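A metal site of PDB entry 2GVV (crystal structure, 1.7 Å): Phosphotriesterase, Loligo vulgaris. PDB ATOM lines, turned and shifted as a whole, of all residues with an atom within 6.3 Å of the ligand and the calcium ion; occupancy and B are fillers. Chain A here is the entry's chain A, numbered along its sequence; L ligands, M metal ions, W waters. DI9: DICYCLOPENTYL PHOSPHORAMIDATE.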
ATOM      1  N   GLY A  19     -11.465  29.297  26.693  1.00  0.00           N
ATOM      2  CA  GLY A  19     -11.063  28.072  26.022  1.00  0.00           C
ATOM      3  C   GLY A  19      -9.757  28.169  25.263  1.00  0.00           C
ATOM      4  O   GLY A  19      -9.563  27.423  24.297  1.00  0.00           O
ATOM      5  N   ALA A  20      -8.863  29.059  25.702  1.00  0.00           N
ATOM      6  CA  ALA A  20      -7.554  29.274  25.077  1.00  0.00           C
ATOM      7  C   ALA A  20      -7.033  28.002  24.421  1.00  0.00           C
ATOM      8  O   ALA A  20      -6.826  26.991  25.075  1.00  0.00           O
ATOM      9  CB  ALA A  20      -6.553  29.772  26.116  1.00  0.00           C
ATOM     10  N   GLU A  21      -6.814  28.077  23.109  1.00  0.00           N
ATOM     11  CA  GLU A  21      -6.354  26.928  22.349  1.00  0.00           C
ATOM     12  C   GLU A  21      -5.466  27.303  21.169  1.00  0.00           C
ATOM     13  O   GLU A  21      -5.156  28.476  20.956  1.00  0.00           O
ATOM     14  CB  GLU A  21      -7.590  26.165  21.832  1.00  0.00           C
ATOM     15  CG  GLU A  21      -7.902  24.876  22.579  1.00  0.00           C
ATOM     16  CD  GLU A  21      -7.186  23.684  21.985  1.00  0.00           C
ATOM     17  OE1 GLU A  21      -6.079  23.877  21.436  1.00  0.00           O
ATOM     18  OE2 GLU A  21      -7.718  22.555  22.082  1.00  0.00           O
ATOM     19  N   PRO A  36     -12.049  29.488  21.265  1.00  0.00           N
ATOM     20  CA  PRO A  36     -13.235  28.766  20.791  1.00  0.00           C
ATOM     21  C   PRO A  36     -14.521  28.950  21.592  1.00  0.00           C
ATOM     22  O   PRO A  36     -15.614  28.796  21.044  1.00  0.00           O
ATOM     23  CB  PRO A  36     -12.775  27.306  20.795  1.00  0.00           C
ATOM     24  CG  PRO A  36     -11.802  27.267  21.933  1.00  0.00           C
ATOM     25  CD  PRO A  36     -11.015  28.543  21.737  1.00  0.00           C
ATOM     26  N   GLU A  37     -14.404  29.302  22.866  1.00  0.00           N
ATOM     27  CA  GLU A  37     -15.570  29.434  23.718  1.00  0.00           C
ATOM     28  C   GLU A  37     -16.209  30.804  23.875  1.00  0.00           C
ATOM     29  O   GLU A  37     -17.052  30.993  24.746  1.00  0.00           O
ATOM     30  CB  GLU A  37     -15.250  28.858  25.100  1.00  0.00           C
ATOM     31  CG  GLU A  37     -14.978  27.375  25.074  1.00  0.00           C
ATOM     32  CD  GLU A  37     -14.674  26.817  26.450  1.00  0.00           C
ATOM     33  OE1 GLU A  37     -15.514  26.981  27.361  1.00  0.00           O
ATOM     34  OE2 GLU A  37     -13.595  26.203  26.622  1.00  0.00           O
ATOM     35  N   ILE A  72     -15.988  28.016  15.860  1.00  0.00           N
ATOM     36  CA  ILE A  72     -15.403  27.596  17.121  1.00  0.00           C
ATOM     37  C   ILE A  72     -13.981  27.166  16.752  1.00  0.00           C
ATOM     38  O   ILE A  72     -13.670  25.977  16.704  1.00  0.00           O
ATOM     39  CB  ILE A  72     -16.188  26.392  17.738  1.00  0.00           C
ATOM     40  CG1 ILE A  72     -17.620  26.828  18.076  1.00  0.00           C
ATOM     41  CG2 ILE A  72     -15.485  25.903  18.995  1.00  0.00           C
ATOM     42  CD1 ILE A  72     -18.474  25.704  18.663  1.00  0.00           C
ATOM     43  N   PRO A  73     -13.107  28.145  16.459  1.00  0.00           N
ATOM     44  CA  PRO A  73     -11.706  27.866  16.099  1.00  0.00           C
ATOM     45  C   PRO A  73     -10.995  27.192  17.253  1.00  0.00           C
ATOM     46  O   PRO A  73     -11.020  27.702  18.372  1.00  0.00           O
ATOM     47  CB  PRO A  73     -11.154  29.242  15.771  1.00  0.00           C
ATOM     48  CG  PRO A  73     -11.968  30.154  16.641  1.00  0.00           C
ATOM     49  CD  PRO A  73     -13.356  29.593  16.501  1.00  0.00           C
ATOM     50  N   ALA A  74     -10.317  26.087  16.984  1.00  0.00           N
ATOM     51  CA  ALA A  74      -9.673  25.335  18.051  1.00  0.00           C
ATOM     52  C   ALA A  74      -8.223  24.920  17.867  1.00  0.00           C
ATOM     53  O   ALA A  74      -7.549  24.617  18.853  1.00  0.00           O
ATOM     54  CB  ALA A  74     -10.504  24.086  18.344  1.00  0.00           C
ATOM     55  N   MET A  90     -14.397  23.798  14.948  1.00  0.00           N
ATOM     56  CA  MET A  90     -15.402  22.792  15.296  1.00  0.00           C
ATOM     57  C   MET A  90     -16.760  22.978  14.615  1.00  0.00           C
ATOM     58  O   MET A  90     -17.562  22.053  14.547  1.00  0.00           O
ATOM     59  CB  MET A  90     -15.587  22.747  16.823  1.00  0.00           C
ATOM     60  CG  MET A  90     -14.382  22.220  17.586  1.00  0.00           C
ATOM     61  SD  MET A  90     -14.196  20.417  17.509  1.00  0.00           S
ATOM     62  CE  MET A  90     -15.343  19.939  18.819  1.00  0.00           C
ATOM     63  N   ASN A 120     -10.753  19.886  15.062  1.00  0.00           N
ATOM     64  CA  ASN A 120     -10.192  20.365  16.323  1.00  0.00           C
ATOM     65  C   ASN A 120      -8.718  20.770  16.279  1.00  0.00           C
ATOM     66  O   ASN A 120      -8.363  21.849  16.746  1.00  0.00           O
ATOM     67  CB  ASN A 120     -10.395  19.291  17.405  1.00  0.00           C
ATOM     68  CG  ASN A 120     -10.066  19.810  18.786  1.00  0.00           C
ATOM     69  OD1 ASN A 120      -8.897  19.920  19.159  1.00  0.00           O
ATOM     70  ND2 ASN A 120     -11.102  20.128  19.553  1.00  0.00           N
ATOM     71  N   ASP A 121      -7.858  19.914  15.733  1.00  0.00           N
ATOM     72  CA  ASP A 121      -6.433  20.248  15.650  1.00  0.00           C
ATOM     73  C   ASP A 121      -5.861  19.733  14.341  1.00  0.00           C
ATOM     74  O   ASP A 121      -6.496  18.949  13.626  1.00  0.00           O
ATOM     75  CB  ASP A 121      -5.665  19.646  16.838  1.00  0.00           C
ATOM     76  CG  ASP A 121      -4.504  20.516  17.299  1.00  0.00           C
ATOM     77  OD1 ASP A 121      -4.071  21.411  16.537  1.00  0.00           O
ATOM     78  OD2 ASP A 121      -4.000  20.304  18.428  1.00  0.00           O
ATOM     79  N   TYR A 144     -24.960  21.369  16.002  1.00  0.00           N
ATOM     80  CA  TYR A 144     -23.697  21.026  16.643  1.00  0.00           C
ATOM     81  C   TYR A 144     -23.738  19.793  17.528  1.00  0.00           C
ATOM     82  O   TYR A 144     -24.597  19.657  18.400  1.00  0.00           O
ATOM     83  CB  TYR A 144     -23.211  22.224  17.474  1.00  0.00           C
ATOM     84  CG  TYR A 144     -21.847  22.031  18.092  1.00  0.00           C
ATOM     85  CD1 TYR A 144     -20.727  21.779  17.293  1.00  0.00           C
ATOM     86  CD2 TYR A 144     -21.667  22.139  19.470  1.00  0.00           C
ATOM     87  CE1 TYR A 144     -19.461  21.649  17.855  1.00  0.00           C
ATOM     88  CE2 TYR A 144     -20.404  22.000  20.047  1.00  0.00           C
ATOM     89  CZ  TYR A 144     -19.309  21.753  19.227  1.00  0.00           C
ATOM     90  OH  TYR A 144     -18.046  21.643  19.786  1.00  0.00           O
ATOM     91  N   MET A 148     -17.890  12.896  22.094  1.00  0.00           N
ATOM     92  CA  MET A 148     -17.349  12.600  23.421  1.00  0.00           C
ATOM     93  C   MET A 148     -17.922  11.288  23.955  1.00  0.00           C
ATOM     94  O   MET A 148     -17.253  10.582  24.719  1.00  0.00           O
ATOM     95  CB  MET A 148     -17.676  13.730  24.400  1.00  0.00           C
ATOM     96  CG  MET A 148     -16.596  14.783  24.528  1.00  0.00           C
ATOM     97  SD  MET A 148     -15.062  14.098  25.202  1.00  0.00           S
ATOM     98  CE  MET A 148     -15.424  14.113  26.954  1.00  0.00           C
ATOM     99  N   PHE A 173     -13.832  11.243  20.041  1.00  0.00           N
ATOM    100  CA  PHE A 173     -13.208  12.537  20.216  1.00  0.00           C
ATOM    101  C   PHE A 173     -11.711  12.619  19.905  1.00  0.00           C
ATOM    102  O   PHE A 173     -10.879  12.788  20.804  1.00  0.00           O
ATOM    103  CB  PHE A 173     -13.464  13.099  21.623  1.00  0.00           C
ATOM    104  CG  PHE A 173     -13.538  14.605  21.660  1.00  0.00           C
ATOM    105  CD1 PHE A 173     -12.373  15.376  21.725  1.00  0.00           C
ATOM    106  CD2 PHE A 173     -14.766  15.261  21.553  1.00  0.00           C
ATOM    107  CE1 PHE A 173     -12.439  16.772  21.680  1.00  0.00           C
ATOM    108  CE2 PHE A 173     -14.831  16.657  21.508  1.00  0.00           C
ATOM    109  CZ  PHE A 173     -13.670  17.406  21.568  1.00  0.00           C
ATOM    110  N   ASN A 175      -8.429  14.270  19.107  1.00  0.00           N
ATOM    111  CA  ASN A 175      -8.072  15.622  19.496  1.00  0.00           C
ATOM    112  C   ASN A 175      -6.707  16.070  18.983  1.00  0.00           C
ATOM    113  O   ASN A 175      -6.583  16.542  17.850  1.00  0.00           O
ATOM    114  CB  ASN A 175      -8.109  15.697  21.035  1.00  0.00           C
ATOM    115  CG  ASN A 175      -8.355  17.081  21.548  1.00  0.00           C
ATOM    116  OD1 ASN A 175      -7.948  18.062  20.932  1.00  0.00           O
ATOM    117  ND2 ASN A 175      -9.009  17.183  22.700  1.00  0.00           N
ATOM    118  N   GLY A 176      -5.686  15.929  19.828  1.00  0.00           N
ATOM    119  CA  GLY A 176      -4.341  16.307  19.427  1.00  0.00           C
ATOM    120  C   GLY A 176      -3.851  15.393  18.322  1.00  0.00           C
ATOM    121  O   GLY A 176      -4.329  14.270  18.175  1.00  0.00           O
ATOM    122  N   THR A 195      -9.204  11.595  23.316  1.00  0.00           N
ATOM    123  CA  THR A 195      -9.333  12.111  24.660  1.00  0.00           C
ATOM    124  C   THR A 195      -9.941  11.284  25.792  1.00  0.00           C
ATOM    125  O   THR A 195      -9.229  10.864  26.702  1.00  0.00           O
ATOM    126  CB  THR A 195     -10.003  13.504  24.626  1.00  0.00           C
ATOM    127  OG1 THR A 195      -9.232  14.361  23.757  1.00  0.00           O
ATOM    128  CG2 THR A 195     -10.040  14.128  26.022  1.00  0.00           C
ATOM    129  N   GLY A 226     -11.439  13.700  31.165  1.00  0.00           N
ATOM    130  CA  GLY A 226     -10.571  14.421  30.259  1.00  0.00           C
ATOM    131  C   GLY A 226      -9.556  13.472  29.652  1.00  0.00           C
ATOM    132  O   GLY A 226      -9.850  12.292  29.456  1.00  0.00           O
ATOM    133  N   GLY A 227      -8.353  13.971  29.369  1.00  0.00           N
ATOM    134  CA  GLY A 227      -7.326  13.136  28.768  1.00  0.00           C
ATOM    135  C   GLY A 227      -6.450  13.946  27.839  1.00  0.00           C
ATOM    136  O   GLY A 227      -6.410  15.167  27.928  1.00  0.00           O
ATOM    137  N   ALA A 228      -5.734  13.273  26.939  1.00  0.00           N
ATOM    138  CA  ALA A 228      -4.848  13.962  26.003  1.00  0.00           C
ATOM    139  C   ALA A 228      -5.569  14.972  25.119  1.00  0.00           C
ATOM    140  O   ALA A 228      -6.586  14.675  24.499  1.00  0.00           O
ATOM    141  CB  ALA A 228      -4.128  12.939  25.132  1.00  0.00           C
ATOM    142  N   ASP A 229      -5.016  16.191  25.076  1.00  0.00           N
ATOM    143  CA  ASP A 229      -5.579  17.257  24.269  1.00  0.00           C
ATOM    144  C   ASP A 229      -4.552  17.566  23.169  1.00  0.00           C
ATOM    145  O   ASP A 229      -4.472  16.834  22.178  1.00  0.00           O
ATOM    146  CB  ASP A 229      -5.826  18.503  25.138  1.00  0.00           C
ATOM    147  CG  ASP A 229      -6.705  19.530  24.450  1.00  0.00           C
ATOM    148  OD1 ASP A 229      -6.773  19.532  23.209  1.00  0.00           O
ATOM    149  OD2 ASP A 229      -7.324  20.362  25.159  1.00  0.00           O
ATOM    150  N   GLY A 230      -3.730  18.600  23.361  1.00  0.00           N
ATOM    151  CA  GLY A 230      -2.737  18.957  22.357  1.00  0.00           C
ATOM    152  C   GLY A 230      -1.367  18.307  22.551  1.00  0.00           C
ATOM    153  O   GLY A 230      -1.029  17.892  23.658  1.00  0.00           O
ATOM    154  N   TRP A 244      -5.313  17.107  29.815  1.00  0.00           N
ATOM    155  CA  TRP A 244      -6.389  17.947  30.325  1.00  0.00           C
ATOM    156  C   TRP A 244      -7.110  17.296  31.509  1.00  0.00           C
ATOM    157  O   TRP A 244      -7.658  16.201  31.403  1.00  0.00           O
ATOM    158  CB  TRP A 244      -7.393  18.208  29.202  1.00  0.00           C
ATOM    159  CG  TRP A 244      -8.344  19.359  29.423  1.00  0.00           C
ATOM    160  CD1 TRP A 244      -8.216  20.628  28.923  1.00  0.00           C
ATOM    161  CD2 TRP A 244      -9.602  19.330  30.113  1.00  0.00           C
ATOM    162  NE1 TRP A 244      -9.324  21.381  29.253  1.00  0.00           N
ATOM    163  CE2 TRP A 244     -10.180  20.609  29.979  1.00  0.00           C
ATOM    164  CE3 TRP A 244     -10.289  18.341  30.831  1.00  0.00           C
ATOM    165  CZ2 TRP A 244     -11.423  20.931  30.542  1.00  0.00           C
ATOM    166  CZ3 TRP A 244     -11.524  18.663  31.388  1.00  0.00           C
ATOM    167  CH2 TRP A 244     -12.076  19.943  31.238  1.00  0.00           C
ATOM    168  N   SER A 271      -4.260  22.558  27.991  1.00  0.00           N
ATOM    169  CA  SER A 271      -4.970  22.220  26.765  1.00  0.00           C
ATOM    170  C   SER A 271      -4.078  22.004  25.552  1.00  0.00           C
ATOM    171  O   SER A 271      -4.120  20.939  24.924  1.00  0.00           O
ATOM    172  CB  SER A 271      -5.997  23.318  26.454  1.00  0.00           C
ATOM    173  OG  SER A 271      -6.636  23.066  25.212  1.00  0.00           O
ATOM    174  N   ASN A 272      -3.276  22.999  25.206  1.00  0.00           N
ATOM    175  CA  ASN A 272      -2.411  22.858  24.044  1.00  0.00           C
ATOM    176  C   ASN A 272      -1.097  23.574  24.277  1.00  0.00           C
ATOM    177  O   ASN A 272      -0.964  24.362  25.213  1.00  0.00           O
ATOM    178  CB  ASN A 272      -3.101  23.409  22.791  1.00  0.00           C
ATOM    179  CG  ASN A 272      -2.809  22.590  21.555  1.00  0.00           C
ATOM    180  OD1 ASN A 272      -1.712  22.059  21.396  1.00  0.00           O
ATOM    181  ND2 ASN A 272      -3.796  22.485  20.661  1.00  0.00           N
ATOM    182  N   HIS A 287      -7.304  25.708  30.542  1.00  0.00           N
ATOM    183  CA  HIS A 287      -8.688  26.082  30.751  1.00  0.00           C
ATOM    184  C   HIS A 287      -9.173  26.256  32.177  1.00  0.00           C
ATOM    185  O   HIS A 287     -10.377  26.380  32.413  1.00  0.00           O
ATOM    186  CB  HIS A 287      -9.574  25.085  30.011  1.00  0.00           C
ATOM    187  CG  HIS A 287      -9.309  25.035  28.548  1.00  0.00           C
ATOM    188  ND1 HIS A 287      -9.824  24.057  27.717  1.00  0.00           N
ATOM    189  CD2 HIS A 287      -8.590  25.854  27.745  1.00  0.00           C
ATOM    190  CE1 HIS A 287      -9.426  24.271  26.480  1.00  0.00           C
ATOM    191  NE2 HIS A 287      -8.673  25.363  26.463  1.00  0.00           N
HETATM  192  CAB DI9 L   1     -10.392  18.435  26.414  1.00  0.00           C
HETATM  193  CAJ DI9 L   1     -11.723  17.969  26.995  1.00  0.00           C
HETATM  194  CAK DI9 L   1     -12.732  18.716  26.120  1.00  0.00           C
HETATM  195  CAL DI9 L   1     -12.099  20.109  26.185  1.00  0.00           C
HETATM  196  CAC DI9 L   1     -10.674  19.780  25.733  1.00  0.00           C
HETATM  197  OAD DI9 L   1     -10.681  19.565  24.323  1.00  0.00           O
HETATM  198  PAE DI9 L   1     -10.300  20.756  23.296  1.00  0.00           P
HETATM  199  NAM DI9 L   1      -9.415  21.817  24.145  1.00  0.00           N
HETATM  200  OAA DI9 L   1      -9.599  20.267  22.091  1.00  0.00           O
HETATM  201  OAF DI9 L   1     -11.684  21.509  22.958  1.00  0.00           O
HETATM  202  CAG DI9 L   1     -11.661  22.817  22.374  1.00  0.00           C
HETATM  203  CAH DI9 L   1     -12.579  22.832  21.156  1.00  0.00           C
HETATM  204  CAI DI9 L   1     -13.944  22.893  21.851  1.00  0.00           C
HETATM  205  CAO DI9 L   1     -13.690  24.095  22.749  1.00  0.00           C
HETATM  206  CAN DI9 L   1     -12.323  23.770  23.366  1.00  0.00           C
HETATM  207 CA    CA M   1      -7.570  20.379  21.155  1.00  0.00          CA
HETATM  208  O   HOH W   1      -5.545  19.466  20.373  1.00  0.00           O
HETATM  209  O   HOH W   2      -6.940  21.923  19.325  1.00  0.00           O
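A nitrogen (NAM) of the ligand sits at hydrogen-bond distance from the side-chain hydroxyl (OG) of Ser 271.
Water W1 bridges the side-chain carboxylate of Asp 121 (2.6 Å) and the backbone carbonyl oxygen of Asp 229 (3.4 Å).
CG of Pro 36 touches CAO of the ligand, at 3.8 Å.
CB of Ala 74 touches CAH of the ligand, 3.7 Å away.
CG of Trp 244 touches CAB of the ligand (3.8 Å).
His 287 touches the ligand.
Hydrophobic or aromatic side chains that line the ligand: Pro 36, Ala 74, Trp 244 and His 287.
Within 4 Å of the ligand: Glu 21, Pro 36, Ala 74, Asn 120, Asn 175, Asp 229, Trp 244, Ser 271 and His 287.
The nearest printed residue that does not touch the ligand is Met 90 (4.05 Å).
OAA of the ligand is bound to the calcium ion (2.2 Å).
The calcium ion is bound by water W1 (2.4 Å).
The calcium ion is bound by OD1 of Asn 175, 2.4 Å away.
OD1 of Asp 229 binds the calcium ion, 2.4 Å away.
The calcium ion is bound by OE2 of Glu 21 (2.4 Å).
The calcium ion is bound by the side-chain amide oxygen (OD1) of Asn 120 (2.4 Å).
The calcium ion is bound by water W2.
The calcium ion has seven donor atoms within binding distance.
Within 4 Å of the calcium ion: Glu 21, Asn 120, Asn 175 and Asp 229.
The backbone carbonyl oxygen of Gly 227 lies within hydrogen-bond range of the backbone NH of Trp 244.
The backbone NH (N) of Gly 230 is in hydrogen-bond range of the backbone carbonyl oxygen (O) of Ser 271 (2.8 Å).
The backbone carbonyl oxygen (O) of Ala 20 is in hydrogen-bond range of a ring nitrogen (NE2) of His 287.
The side-chain hydroxyl (OG1) of Thr 195 sits at hydrogen-bond distance from the side-chain amide nitrogen (ND2) of Asn 175 (3.0 Å).
The side-chain amide nitrogen of Asn 120 lies within hydrogen-bond range of the side-chain sulfur of Met 90, at 3.7 Å.
The backbone carbonyl oxygen of Asp 229 lies within hydrogen-bond range of the backbone NH of Gly 176, 2.8 Å away.
The side-chain hydroxyl of Ser 271 lies close to a ring nitrogen (NE2) of His 287 (3.3 Å).
A ring nitrogen (ND1) of His 287 lies within hydrogen-bond range of the indole nitrogen of Trp 244, at 3.1 Å.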
